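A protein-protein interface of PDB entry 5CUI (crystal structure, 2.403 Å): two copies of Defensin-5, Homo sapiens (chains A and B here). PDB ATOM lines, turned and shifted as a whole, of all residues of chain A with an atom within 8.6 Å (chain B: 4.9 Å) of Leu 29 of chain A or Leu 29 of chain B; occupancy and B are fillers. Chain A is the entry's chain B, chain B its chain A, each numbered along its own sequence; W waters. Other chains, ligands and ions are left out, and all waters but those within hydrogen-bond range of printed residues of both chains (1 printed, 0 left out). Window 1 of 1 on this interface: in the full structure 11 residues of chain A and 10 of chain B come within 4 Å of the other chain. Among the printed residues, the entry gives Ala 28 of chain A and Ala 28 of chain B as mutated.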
ATOM      1  N   ALA A   1      -5.495 -19.682 -24.462  1.00  0.00           N
ATOM      2  CA  ALA A   1      -4.654 -18.622 -25.004  1.00  0.00           C
ATOM      3  C   ALA A   1      -4.606 -17.394 -24.087  1.00  0.00           C
ATOM      4  O   ALA A   1      -5.387 -17.256 -23.151  1.00  0.00           O
ATOM      5  CB  ALA A   1      -5.132 -18.214 -26.402  1.00  0.00           C
ATOM      6  N   THR A   2      -3.677 -16.495 -24.382  1.00  0.00           N
ATOM      7  CA  THR A   2      -3.572 -15.237 -23.659  1.00  0.00           C
ATOM      8  C   THR A   2      -4.242 -14.155 -24.487  1.00  0.00           C
ATOM      9  O   THR A   2      -3.836 -13.896 -25.612  1.00  0.00           O
ATOM     10  CB  THR A   2      -2.112 -14.874 -23.369  1.00  0.00           C
ATOM     11  OG1 THR A   2      -1.580 -15.834 -22.456  1.00  0.00           O
ATOM     12  CG2 THR A   2      -1.996 -13.484 -22.752  1.00  0.00           C
ATOM     13  N   CYS A   3      -5.294 -13.556 -23.934  1.00  0.00           N
ATOM     14  CA  CYS A   3      -6.155 -12.655 -24.696  1.00  0.00           C
ATOM     15  C   CYS A   3      -6.479 -11.439 -23.874  1.00  0.00           C
ATOM     16  O   CYS A   3      -6.559 -11.506 -22.653  1.00  0.00           O
ATOM     17  CB  CYS A   3      -7.457 -13.348 -25.135  1.00  0.00           C
ATOM     18  SG  CYS A   3      -7.285 -14.712 -26.314  1.00  0.00           S
ATOM     19  N   TYR A   4      -6.649 -10.321 -24.561  1.00  0.00           N
ATOM     20  CA  TYR A   4      -6.999  -9.061 -23.921  1.00  0.00           C
ATOM     21  C   TYR A   4      -8.175  -8.419 -24.646  1.00  0.00           C
ATOM     22  O   TYR A   4      -8.418  -8.665 -25.845  1.00  0.00           O
ATOM     23  CB  TYR A   4      -5.800  -8.111 -23.896  1.00  0.00           C
ATOM     24  CG  TYR A   4      -4.631  -8.675 -23.122  1.00  0.00           C
ATOM     25  CD1 TYR A   4      -3.476  -9.096 -23.773  1.00  0.00           C
ATOM     26  CD2 TYR A   4      -4.697  -8.820 -21.737  1.00  0.00           C
ATOM     27  CE1 TYR A   4      -2.422  -9.623 -23.065  1.00  0.00           C
ATOM     28  CE2 TYR A   4      -3.642  -9.340 -21.020  1.00  0.00           C
ATOM     29  CZ  TYR A   4      -2.507  -9.746 -21.686  1.00  0.00           C
ATOM     30  OH  TYR A   4      -1.442 -10.267 -20.975  1.00  0.00           O
ATOM     31  N   CYS A   5      -8.922  -7.615 -23.906  1.00  0.00           N
ATOM     32  CA  CYS A   5     -10.061  -6.932 -24.480  1.00  0.00           C
ATOM     33  C   CYS A   5      -9.688  -5.480 -24.656  1.00  0.00           C
ATOM     34  O   CYS A   5      -9.641  -4.730 -23.693  1.00  0.00           O
ATOM     35  CB  CYS A   5     -11.309  -7.134 -23.602  1.00  0.00           C
ATOM     36  SG  CYS A   5     -11.978  -8.842 -23.730  1.00  0.00           S
ATOM     37  N   ARG A   6      -9.416  -5.097 -25.898  1.00  0.00           N
ATOM     38  CA  ARG A   6      -8.753  -3.818 -26.192  1.00  0.00           C
ATOM     39  C   ARG A   6      -9.660  -2.698 -26.697  1.00  0.00           C
ATOM     40  O   ARG A   6     -10.595  -2.930 -27.450  1.00  0.00           O
ATOM     41  CB  ARG A   6      -7.633  -4.040 -27.203  1.00  0.00           C
ATOM     42  CG  ARG A   6      -6.519  -4.906 -26.657  1.00  0.00           C
ATOM     43  CD  ARG A   6      -5.172  -4.502 -27.255  1.00  0.00           C
ATOM     44  NE  ARG A   6      -4.061  -5.198 -26.634  1.00  0.00           N
ATOM     45  CZ  ARG A   6      -3.434  -4.790 -25.535  1.00  0.00           C
ATOM     46  NH1 ARG A   6      -3.804  -3.672 -24.928  1.00  0.00           N
ATOM     47  NH2 ARG A   6      -2.420  -5.502 -25.057  1.00  0.00           N
ATOM     48  N   THR A   7      -9.362  -1.478 -26.272  1.00  0.00           N
ATOM     49  CA  THR A   7     -10.066  -0.303 -26.763  1.00  0.00           C
ATOM     50  C   THR A   7      -9.368   0.247 -28.005  1.00  0.00           C
ATOM     51  O   THR A   7      -9.937   1.045 -28.740  1.00  0.00           O
ATOM     52  CB  THR A   7     -10.144   0.805 -25.704  1.00  0.00           C
ATOM     53  OG1 THR A   7      -8.818   1.231 -25.381  1.00  0.00           O
ATOM     54  CG2 THR A   7     -10.851   0.302 -24.443  1.00  0.00           C
ATOM     55  N   GLY A   8      -8.128  -0.177 -28.225  1.00  0.00           N
ATOM     56  CA  GLY A   8      -7.390   0.231 -29.399  1.00  0.00           C
ATOM     57  C   GLY A   8      -7.057  -0.953 -30.287  1.00  0.00           C
ATOM     58  O   GLY A   8      -7.678  -2.020 -30.195  1.00  0.00           O
ATOM     59  N   ARG A   9      -6.060  -0.760 -31.146  1.00  0.00           N
ATOM     60  CA  ARG A   9      -5.564  -1.823 -32.006  1.00  0.00           C
ATOM     61  C   ARG A   9      -4.776  -2.863 -31.208  1.00  0.00           C
ATOM     62  O   ARG A   9      -4.273  -2.581 -30.123  1.00  0.00           O
ATOM     63  CB  ARG A   9      -4.677  -1.239 -33.101  1.00  0.00           C
ATOM     64  CG  ARG A   9      -3.413  -0.608 -32.539  1.00  0.00           C
ATOM     65  CD  ARG A   9      -2.523  -0.023 -33.612  1.00  0.00           C
ATOM     66  NE  ARG A   9      -1.307   0.527 -33.020  1.00  0.00           N
ATOM     67  CZ  ARG A   9      -0.205  -0.178 -32.783  1.00  0.00           C
ATOM     68  NH1 ARG A   9      -0.160  -1.469 -33.080  1.00  0.00           N
ATOM     69  NH2 ARG A   9       0.854   0.409 -32.243  1.00  0.00           N
ATOM     70  N   CYS A  10      -4.665  -4.061 -31.765  1.00  0.00           N
ATOM     71  CA  CYS A  10      -3.888  -5.120 -31.153  1.00  0.00           C
ATOM     72  C   CYS A  10      -2.408  -4.793 -31.178  1.00  0.00           C
ATOM     73  O   CYS A  10      -1.912  -4.177 -32.125  1.00  0.00           O
ATOM     74  CB  CYS A  10      -4.164  -6.449 -31.860  1.00  0.00           C
ATOM     75  SG  CYS A  10      -5.911  -6.985 -31.665  1.00  0.00           S
ATOM     76  N   GLU A  14      -0.002  -9.637 -31.099  1.00  0.00           N
ATOM     77  CA  GLU A  14      -1.361 -10.117 -30.916  1.00  0.00           C
ATOM     78  C   GLU A  14      -2.056 -10.188 -32.265  1.00  0.00           C
ATOM     79  O   GLU A  14      -1.662  -9.509 -33.215  1.00  0.00           O
ATOM     80  CB  GLU A  14      -2.138  -9.205 -29.963  1.00  0.00           C
ATOM     81  CG  GLU A  14      -1.531  -9.095 -28.580  1.00  0.00           C
ATOM     82  CD  GLU A  14      -2.114  -7.947 -27.764  1.00  0.00           C
ATOM     83  OE1 GLU A  14      -2.887  -7.141 -28.322  1.00  0.00           O
ATOM     84  OE2 GLU A  14      -1.796  -7.835 -26.562  1.00  0.00           O
ATOM     85  N   SER A  15      -3.082 -11.028 -32.345  1.00  0.00           N
ATOM     86  CA  SER A  15      -3.976 -11.061 -33.499  1.00  0.00           C
ATOM     87  C   SER A  15      -5.391 -10.682 -33.088  1.00  0.00           C
ATOM     88  O   SER A  15      -5.881 -11.120 -32.052  1.00  0.00           O
ATOM     89  CB  SER A  15      -3.989 -12.441 -34.145  1.00  0.00           C
ATOM     90  OG  SER A  15      -2.695 -12.781 -34.572  1.00  0.00           O
ATOM     91  N   LEU A  16      -6.026  -9.852 -33.909  1.00  0.00           N
ATOM     92  CA  LEU A  16      -7.434  -9.531 -33.762  1.00  0.00           C
ATOM     93  C   LEU A  16      -8.247 -10.798 -34.006  1.00  0.00           C
ATOM     94  O   LEU A  16      -8.204 -11.358 -35.098  1.00  0.00           O
ATOM     95  CB  LEU A  16      -7.830  -8.423 -34.737  1.00  0.00           C
ATOM     96  CG  LEU A  16      -9.268  -7.912 -34.617  1.00  0.00           C
ATOM     97  CD1 LEU A  16      -9.527  -7.385 -33.206  1.00  0.00           C
ATOM     98  CD2 LEU A  16      -9.538  -6.833 -35.673  1.00  0.00           C
ATOM     99  N   SER A  17      -8.976 -11.250 -32.991  1.00  0.00           N
ATOM    100  CA  SER A  17      -9.577 -12.579 -33.027  1.00  0.00           C
ATOM    101  C   SER A  17     -11.086 -12.582 -32.836  1.00  0.00           C
ATOM    102  O   SER A  17     -11.717 -13.624 -32.962  1.00  0.00           O
ATOM    103  CB  SER A  17      -8.942 -13.473 -31.955  1.00  0.00           C
ATOM    104  OG  SER A  17      -7.536 -13.562 -32.114  1.00  0.00           O
ATOM    105  N   GLY A  18     -11.660 -11.428 -32.512  1.00  0.00           N
ATOM    106  CA  GLY A  18     -13.088 -11.338 -32.306  1.00  0.00           C
ATOM    107  C   GLY A  18     -13.485 -10.119 -31.523  1.00  0.00           C
ATOM    108  O   GLY A  18     -12.779  -9.104 -31.570  1.00  0.00           O
ATOM    109  N   VAL A  19     -14.613 -10.208 -30.812  1.00  0.00           N
ATOM    110  CA  VAL A  19     -15.053  -9.103 -29.957  1.00  0.00           C
ATOM    111  C   VAL A  19     -15.398  -9.550 -28.540  1.00  0.00           C
ATOM    112  O   VAL A  19     -15.933 -10.637 -28.318  1.00  0.00           O
ATOM    113  CB  VAL A  19     -16.298  -8.340 -30.558  1.00  0.00           C
ATOM    114  CG1 VAL A  19     -15.983  -7.800 -31.928  1.00  0.00           C
ATOM    115  CG2 VAL A  19     -17.553  -9.208 -30.585  1.00  0.00           C
ATOM    116  N   CYS A  20     -15.082  -8.688 -27.582  1.00  0.00           N
ATOM    117  CA  CYS A  20     -15.443  -8.897 -26.182  1.00  0.00           C
ATOM    118  C   CYS A  20     -16.649  -8.070 -25.860  1.00  0.00           C
ATOM    119  O   CYS A  20     -16.768  -6.933 -26.314  1.00  0.00           O
ATOM    120  CB  CYS A  20     -14.324  -8.483 -25.234  1.00  0.00           C
ATOM    121  SG  CYS A  20     -12.719  -9.090 -25.638  1.00  0.00           S
ATOM    122  N   GLU A  21     -17.540  -8.639 -25.066  1.00  0.00           N
ATOM    123  CA  GLU A  21     -18.703  -7.920 -24.585  1.00  0.00           C
ATOM    124  C   GLU A  21     -18.681  -8.000 -23.075  1.00  0.00           C
ATOM    125  O   GLU A  21     -18.996  -9.027 -22.493  1.00  0.00           O
ATOM    126  CB  GLU A  21     -19.987  -8.506 -25.158  1.00  0.00           C
ATOM    127  CG  GLU A  21     -20.093  -8.383 -26.647  1.00  0.00           C
ATOM    128  CD  GLU A  21     -21.459  -8.784 -27.156  1.00  0.00           C
ATOM    129  OE1 GLU A  21     -22.224  -9.415 -26.389  1.00  0.00           O
ATOM    130  OE2 GLU A  21     -21.765  -8.464 -28.323  1.00  0.00           O
ATOM    131  N   ILE A  22     -18.259  -6.915 -22.450  1.00  0.00           N
ATOM    132  CA  ILE A  22     -18.038  -6.888 -21.020  1.00  0.00           C
ATOM    133  C   ILE A  22     -18.760  -5.687 -20.456  1.00  0.00           C
ATOM    134  O   ILE A  22     -18.414  -4.558 -20.799  1.00  0.00           O
ATOM    135  CB  ILE A  22     -16.539  -6.778 -20.668  1.00  0.00           C
ATOM    136  CG1 ILE A  22     -15.675  -7.656 -21.574  1.00  0.00           C
ATOM    137  CG2 ILE A  22     -16.320  -7.162 -19.221  1.00  0.00           C
ATOM    138  CD1 ILE A  22     -15.783  -9.120 -21.274  1.00  0.00           C
ATOM    139  N   LEU A  26     -18.444  -2.918 -26.059  1.00  0.00           N
ATOM    140  CA  LEU A  26     -17.687  -3.650 -27.069  1.00  0.00           C
ATOM    141  C   LEU A  26     -16.175  -3.408 -26.966  1.00  0.00           C
ATOM    142  O   LEU A  26     -15.736  -2.290 -26.694  1.00  0.00           O
ATOM    143  CB  LEU A  26     -18.163  -3.243 -28.456  1.00  0.00           C
ATOM    144  CG  LEU A  26     -19.607  -3.615 -28.761  1.00  0.00           C
ATOM    145  CD1 LEU A  26     -20.213  -2.687 -29.840  1.00  0.00           C
ATOM    146  CD2 LEU A  26     -19.666  -5.092 -29.161  1.00  0.00           C
ATOM    147  N   TYR A  27     -15.385  -4.458 -27.189  1.00  0.00           N
ATOM    148  CA  TYR A  27     -13.936  -4.336 -27.253  1.00  0.00           C
ATOM    149  C   TYR A  27     -13.395  -5.278 -28.317  1.00  0.00           C
ATOM    150  O   TYR A  27     -14.027  -6.264 -28.680  1.00  0.00           O
ATOM    151  CB  TYR A  27     -13.281  -4.649 -25.893  1.00  0.00           C
ATOM    152  CG  TYR A  27     -13.802  -3.842 -24.715  1.00  0.00           C
ATOM    153  CD1 TYR A  27     -14.825  -4.336 -23.898  1.00  0.00           C
ATOM    154  CD2 TYR A  27     -13.265  -2.602 -24.405  1.00  0.00           C
ATOM    155  CE1 TYR A  27     -15.300  -3.613 -22.826  1.00  0.00           C
ATOM    156  CE2 TYR A  27     -13.741  -1.865 -23.332  1.00  0.00           C
ATOM    157  CZ  TYR A  27     -14.754  -2.376 -22.545  1.00  0.00           C
ATOM    158  OH  TYR A  27     -15.216  -1.642 -21.475  1.00  0.00           O
ATOM    159  N   ALA A  28     -12.207  -4.979 -28.811  1.00  0.00           N
ATOM    160  CA  ALA A  28     -11.556  -5.869 -29.748  1.00  0.00           C
ATOM    161  C   ALA A  28     -10.895  -6.993 -28.961  1.00  0.00           C
ATOM    162  O   ALA A  28     -10.218  -6.741 -27.963  1.00  0.00           O
ATOM    163  CB  ALA A  28     -10.552  -5.112 -30.584  1.00  0.00           C
ATOM    164  N   LEU A  29     -11.132  -8.232 -29.383  1.00  0.00           N
ATOM    165  CA  LEU A  29     -10.480  -9.380 -28.774  1.00  0.00           C
ATOM    166  C   LEU A  29      -9.106  -9.567 -29.423  1.00  0.00           C
ATOM    167  O   LEU A  29      -9.010  -9.818 -30.626  1.00  0.00           O
ATOM    168  CB  LEU A  29     -11.342 -10.644 -28.917  1.00  0.00           C
ATOM    169  CG  LEU A  29     -10.650 -11.968 -28.574  1.00  0.00           C
ATOM    170  CD1 LEU A  29     -10.270 -12.011 -27.074  1.00  0.00           C
ATOM    171  CD2 LEU A  29     -11.460 -13.215 -29.011  1.00  0.00           C
ATOM    172  N   CYS A  30      -8.044  -9.410 -28.629  1.00  0.00           N
ATOM    173  CA  CYS A  30      -6.665  -9.522 -29.136  1.00  0.00           C
ATOM    174  C   CYS A  30      -5.904 -10.670 -28.459  1.00  0.00           C
ATOM    175  O   CYS A  30      -5.732 -10.691 -27.242  1.00  0.00           O
ATOM    176  CB  CYS A  30      -5.903  -8.201 -28.940  1.00  0.00           C
ATOM    177  SG  CYS A  30      -6.683  -6.778 -29.767  1.00  0.00           S
ATOM    178  N   CYS A  31      -5.432 -11.615 -29.261  1.00  0.00           N
ATOM    179  CA  CYS A  31      -4.903 -12.856 -28.716  1.00  0.00           C
ATOM    180  C   CYS A  31      -3.476 -13.146 -29.155  1.00  0.00           C
ATOM    181  O   CYS A  31      -3.061 -12.776 -30.252  1.00  0.00           O
ATOM    182  CB  CYS A  31      -5.824 -14.026 -29.108  1.00  0.00           C
ATOM    183  SG  CYS A  31      -7.436 -14.034 -28.257  1.00  0.00           S
ATOM    184  N   ARG A  32      -2.725 -13.811 -28.284  1.00  0.00           N
ATOM    185  CA  ARG A  32      -1.400 -14.280 -28.640  1.00  0.00           C
ATOM    186  C   ARG A  32      -1.156 -15.689 -28.134  1.00  0.00           C
ATOM    187  O   ARG A  32      -0.166 -16.313 -28.525  1.00  0.00           O
ATOM    188  CB  ARG A  32      -0.334 -13.336 -28.102  1.00  0.00           C
ATOM    189  CG  ARG A  32      -0.360 -13.099 -26.602  1.00  0.00           C
ATOM    190  CD  ARG A  32       0.884 -12.324 -26.230  1.00  0.00           C
ATOM    191  NE  ARG A  32       0.872 -11.809 -24.868  1.00  0.00           N
ATOM    192  CZ  ARG A  32       1.328 -12.475 -23.812  1.00  0.00           C
ATOM    193  NH1 ARG A  32       1.813 -13.698 -23.954  1.00  0.00           N
ATOM    194  NH2 ARG A  32       1.288 -11.918 -22.610  1.00  0.00           N
ATOM    195  OXT ARG A  32      -1.924 -16.236 -27.337  1.00  0.00           O
ATOM    196  N   CYS B   3      -8.081 -17.430 -22.201  1.00  0.00           N
ATOM    197  CA  CYS B   3      -9.326 -17.470 -22.949  1.00  0.00           C
ATOM    198  C   CYS B   3      -9.306 -18.548 -24.013  1.00  0.00           C
ATOM    199  O   CYS B   3      -8.259 -18.879 -24.572  1.00  0.00           O
ATOM    200  CB  CYS B   3      -9.613 -16.114 -23.608  1.00  0.00           C
ATOM    201  SG  CYS B   3      -9.924 -14.722 -22.493  1.00  0.00           S
ATOM    202  N   TYR B   4     -10.488 -19.081 -24.295  1.00  0.00           N
ATOM    203  CA  TYR B   4     -10.644 -20.094 -25.319  1.00  0.00           C
ATOM    204  C   TYR B   4     -11.763 -19.723 -26.285  1.00  0.00           C
ATOM    205  O   TYR B   4     -12.770 -19.092 -25.905  1.00  0.00           O
ATOM    206  CB  TYR B   4     -10.912 -21.452 -24.676  1.00  0.00           C
ATOM    207  CG  TYR B   4      -9.845 -21.861 -23.684  1.00  0.00           C
ATOM    208  CD1 TYR B   4     -10.089 -21.814 -22.314  1.00  0.00           C
ATOM    209  CD2 TYR B   4      -8.583 -22.268 -24.116  1.00  0.00           C
ATOM    210  CE1 TYR B   4      -9.112 -22.186 -21.399  1.00  0.00           C
ATOM    211  CE2 TYR B   4      -7.598 -22.644 -23.209  1.00  0.00           C
ATOM    212  CZ  TYR B   4      -7.875 -22.598 -21.852  1.00  0.00           C
ATOM    213  OH  TYR B   4      -6.916 -22.967 -20.946  1.00  0.00           O
ATOM    214  N   CYS B   5     -11.564 -20.114 -27.538  1.00  0.00           N
ATOM    215  CA  CYS B   5     -12.583 -19.979 -28.566  1.00  0.00           C
ATOM    216  C   CYS B   5     -13.306 -21.301 -28.731  1.00  0.00           C
ATOM    217  O   CYS B   5     -12.770 -22.254 -29.298  1.00  0.00           O
ATOM    218  CB  CYS B   5     -11.957 -19.530 -29.879  1.00  0.00           C
ATOM    219  SG  CYS B   5     -11.293 -17.872 -29.758  1.00  0.00           S
ATOM    220  N   CYS B  10     -19.351 -22.629 -22.504  1.00  0.00           N
ATOM    221  CA  CYS B  10     -18.183 -22.413 -21.658  1.00  0.00           C
ATOM    222  C   CYS B  10     -18.163 -23.457 -20.547  1.00  0.00           C
ATOM    223  O   CYS B  10     -19.219 -23.958 -20.133  1.00  0.00           O
ATOM    224  CB  CYS B  10     -18.181 -20.989 -21.077  1.00  0.00           C
ATOM    225  SG  CYS B  10     -18.132 -19.726 -22.362  1.00  0.00           S
ATOM    226  N   SER B  15     -16.067 -17.804 -18.024  1.00  0.00           N
ATOM    227  CA  SER B  15     -17.102 -16.797 -18.265  1.00  0.00           C
ATOM    228  C   SER B  15     -17.224 -16.455 -19.736  1.00  0.00           C
ATOM    229  O   SER B  15     -16.230 -16.111 -20.400  1.00  0.00           O
ATOM    230  CB  SER B  15     -16.825 -15.500 -17.504  1.00  0.00           C
ATOM    231  OG  SER B  15     -16.779 -15.739 -16.119  1.00  0.00           O
ATOM    232  N   LEU B  16     -18.460 -16.534 -20.217  1.00  0.00           N
ATOM    233  CA  LEU B  16     -18.816 -16.123 -21.555  1.00  0.00           C
ATOM    234  C   LEU B  16     -18.561 -14.636 -21.707  1.00  0.00           C
ATOM    235  O   LEU B  16     -19.128 -13.844 -20.976  1.00  0.00           O
ATOM    236  CB  LEU B  16     -20.281 -16.459 -21.818  1.00  0.00           C
ATOM    237  CG  LEU B  16     -20.796 -16.160 -23.214  1.00  0.00           C
ATOM    238  CD1 LEU B  16     -19.958 -16.905 -24.262  1.00  0.00           C
ATOM    239  CD2 LEU B  16     -22.278 -16.558 -23.266  1.00  0.00           C
ATOM    240  N   SER B  17     -17.714 -14.253 -22.654  1.00  0.00           N
ATOM    241  CA  SER B  17     -17.203 -12.888 -22.680  1.00  0.00           C
ATOM    242  C   SER B  17     -17.255 -12.250 -24.051  1.00  0.00           C
ATOM    243  O   SER B  17     -16.775 -11.144 -24.231  1.00  0.00           O
ATOM    244  CB  SER B  17     -15.753 -12.848 -22.183  1.00  0.00           C
ATOM    245  OG  SER B  17     -15.617 -13.443 -20.907  1.00  0.00           O
ATOM    246  N   GLY B  18     -17.788 -12.960 -25.029  1.00  0.00           N
ATOM    247  CA  GLY B  18     -17.905 -12.406 -26.359  1.00  0.00           C
ATOM    248  C   GLY B  18     -17.819 -13.485 -27.416  1.00  0.00           C
ATOM    249  O   GLY B  18     -18.201 -14.630 -27.187  1.00  0.00           O
ATOM    250  N   VAL B  19     -17.279 -13.110 -28.571  1.00  0.00           N
ATOM    251  CA  VAL B  19     -17.244 -13.976 -29.733  1.00  0.00           C
ATOM    252  C   VAL B  19     -15.876 -13.974 -30.391  1.00  0.00           C
ATOM    253  O   VAL B  19     -15.220 -12.934 -30.486  1.00  0.00           O
ATOM    254  CB  VAL B  19     -18.337 -13.544 -30.757  1.00  0.00           C
ATOM    255  CG1 VAL B  19     -18.115 -14.178 -32.120  1.00  0.00           C
ATOM    256  CG2 VAL B  19     -19.692 -13.915 -30.225  1.00  0.00           C
ATOM    257  N   CYS B  20     -15.438 -15.152 -30.824  1.00  0.00           N
ATOM    258  CA  CYS B  20     -14.279 -15.270 -31.702  1.00  0.00           C
ATOM    259  C   CYS B  20     -14.739 -15.371 -33.144  1.00  0.00           C
ATOM    260  O   CYS B  20     -15.712 -16.060 -33.440  1.00  0.00           O
ATOM    261  CB  CYS B  20     -13.434 -16.501 -31.363  1.00  0.00           C
ATOM    262  SG  CYS B  20     -12.929 -16.647 -29.661  1.00  0.00           S
ATOM    263  N   TYR B  27     -17.166 -18.466 -32.712  1.00  0.00           N
ATOM    264  CA  TYR B  27     -16.905 -19.264 -31.519  1.00  0.00           C
ATOM    265  C   TYR B  27     -17.343 -18.480 -30.297  1.00  0.00           C
ATOM    266  O   TYR B  27     -17.298 -17.259 -30.296  1.00  0.00           O
ATOM    267  CB  TYR B  27     -15.411 -19.632 -31.411  1.00  0.00           C
ATOM    268  CG  TYR B  27     -14.891 -20.409 -32.599  1.00  0.00           C
ATOM    269  CD1 TYR B  27     -14.482 -19.756 -33.765  1.00  0.00           C
ATOM    270  CD2 TYR B  27     -14.814 -21.804 -32.563  1.00  0.00           C
ATOM    271  CE1 TYR B  27     -14.013 -20.469 -34.864  1.00  0.00           C
ATOM    272  CE2 TYR B  27     -14.349 -22.516 -33.642  1.00  0.00           C
ATOM    273  CZ  TYR B  27     -13.950 -21.847 -34.792  1.00  0.00           C
ATOM    274  OH  TYR B  27     -13.486 -22.570 -35.865  1.00  0.00           O
ATOM    275  N   ALA B  28     -17.772 -19.174 -29.252  1.00  0.00           N
ATOM    276  CA  ALA B  28     -17.976 -18.503 -27.976  1.00  0.00           C
ATOM    277  C   ALA B  28     -16.611 -18.152 -27.401  1.00  0.00           C
ATOM    278  O   ALA B  28     -15.663 -18.950 -27.490  1.00  0.00           O
ATOM    279  CB  ALA B  28     -18.764 -19.370 -27.010  1.00  0.00           C
ATOM    280  N   LEU B  29     -16.510 -16.954 -26.836  1.00  0.00           N
ATOM    281  CA  LEU B  29     -15.321 -16.540 -26.099  1.00  0.00           C
ATOM    282  C   LEU B  29     -15.502 -16.887 -24.618  1.00  0.00           C
ATOM    283  O   LEU B  29     -16.445 -16.439 -23.967  1.00  0.00           O
ATOM    284  CB  LEU B  29     -15.051 -15.036 -26.289  1.00  0.00           C
ATOM    285  CG  LEU B  29     -13.916 -14.443 -25.455  1.00  0.00           C
ATOM    286  CD1 LEU B  29     -12.577 -15.105 -25.815  1.00  0.00           C
ATOM    287  CD2 LEU B  29     -13.870 -12.909 -25.580  1.00  0.00           C
ATOM    288  N   CYS B  30     -14.610 -17.717 -24.099  1.00  0.00           N
ATOM    289  CA  CYS B  30     -14.726 -18.208 -22.729  1.00  0.00           C
ATOM    290  C   CYS B  30     -13.420 -17.933 -21.994  1.00  0.00           C
ATOM    291  O   CYS B  30     -12.374 -18.490 -22.321  1.00  0.00           O
ATOM    292  CB  CYS B  30     -15.063 -19.704 -22.702  1.00  0.00           C
ATOM    293  SG  CYS B  30     -16.581 -20.163 -23.631  1.00  0.00           S
ATOM    294  N   CYS B  31     -13.488 -17.045 -21.011  1.00  0.00           N
ATOM    295  CA  CYS B  31     -12.303 -16.620 -20.285  1.00  0.00           C
ATOM    296  C   CYS B  31     -12.334 -17.052 -18.830  1.00  0.00           C
ATOM    297  O   CYS B  31     -13.393 -17.311 -18.257  1.00  0.00           O
ATOM    298  CB  CYS B  31     -12.158 -15.095 -20.398  1.00  0.00           C
ATOM    299  SG  CYS B  31     -11.975 -14.564 -22.150  1.00  0.00           S
HETATM  300  O   HOH W   1     -19.597 -10.483 -20.273  1.00  0.00           O
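The backbone NH (N) of Val 19 of chain A lies within hydrogen-bond range of the backbone carbonyl oxygen (O) of Val 19 of chain B (2.8 Å). O of Ala 1 of chain A sits at hydrogen-bond distance from N of Cys 3 of chain B. The backbone carbonyl oxygen of Ser 17 of chain B sits at hydrogen-bond distance from the backbone NH of Glu 21 of chain A, at 2.7 Å.
N of Cys 20 of chain A is in hydrogen-bond range of O of Tyr 27 of chain A, at 2.9 Å. The side-chain sulfur (SG) of Cys 31 of chain B is disulfide-bonded to the side-chain sulfur (SG) of Cys 3 of chain B (2.1 Å). N of Ser 17 of chain B lies within hydrogen-bond range of O of Leu 29 of chain B, 2.8 Å away. O of Ser 15 of chain B is in hydrogen-bond range of OG of Ser 17 of chain B (2.8 Å). OG of Ser 17 of chain A lies within hydrogen-bond range of O of Ser 15 of chain A. SG of Cys 10 of chain A is disulfide-bonded to SG of Cys 30 of chain A, at 2.1 Å.
Among the printed residues, merely in contact across the chains: Ala 1 of chain A with Tyr 4 of chain B, Cys 3 of chain A with Cys 3 of chain B, Ser 17 of chain A with Cys 20 of chain B, Gly 18 of chain A with Val 19 of chain B, Val 19 of chain A with Gly 18 of chain B, Cys 20 of chain A with Ser 17 of chain B, Cys 20 of chain A with Leu 29 of chain B, Glu 21 of chain A with Gly 18 of chain B, Ile 22 of chain A with Ser 17 of chain B, Leu 29 of chain A with Cys 20 of chain B and Leu 29 of chain A with Leu 29 of chain B.
Printed residues of chain B within 4 Å of Ala 1 of chain A: Cys 3 (2.9 Å) and Tyr 4 (3.8 Å). Printed residues of chain B within 4 Å of Ser 17 of chain A: Cys 20. Of the printed residues of chain B, Gly 18 of chain A touches Val 19. Of the printed residues of chain A, Cys 3 of chain B touches Ala 1 and Cys 3. Printed residues of chain A within 4 Å of Tyr 4 of chain B: Ala 1 (3.8 Å). Of the printed residues of chain A, Ser 17 of chain B touches Cys 20 (3.3 Å), Glu 21 (2.7 Å) and Ile 22 (3.7 Å). No residue of chain A comes within 4 Å of Ala 28 of chain B. Of the printed residues of chain A, Leu 29 of chain B touches Cys 20 and Leu 29. No residue of chain A comes within 4 Å of Cys 30 of chain B. The nearest printed residue of chain B that does not touch Ala 1 of chain A is Cys 5 of chain B (6.8 Å).
Of the 15 printed residues of chain B, 7 touch a printed residue of chain A. Printed residues of chain A that touch a printed residue of chain B: Ala 1, Cys 3, Ser 17, Gly 18, Val 19, Cys 20, Glu 21, Ile 22 and Leu 29. Hydrophobic or aromatic side chains of chain A within 4 Å of the printed part of chain B: Ala 1, Ile 22 and Leu 29. Along chain A the printed residues that touch a printed residue of chain B span positions 1 to 29.
Ser 17 of chain A touches Cys 20 of chain B, and with the chains exchanged Cys 20 of chain A touches Ser 17 of chain B. Gly 18 of chain A touches Val 19 of chain B, and with the chains exchanged Val 19 of chain A touches Gly 18 of chain B. Cys 20 of chain A touches Leu 29 of chain B, and with the chains exchanged Leu 29 of chain A touches Cys 20 of chain B. Leu 29 of chain B touches its own counterpart, Leu 29 of chain A. 15 positions are printed for both chains.
Water W1 bridges O of Glu 21 of chain A (2.7 Å) and O of Leu 16 of chain B (3.5 Å).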
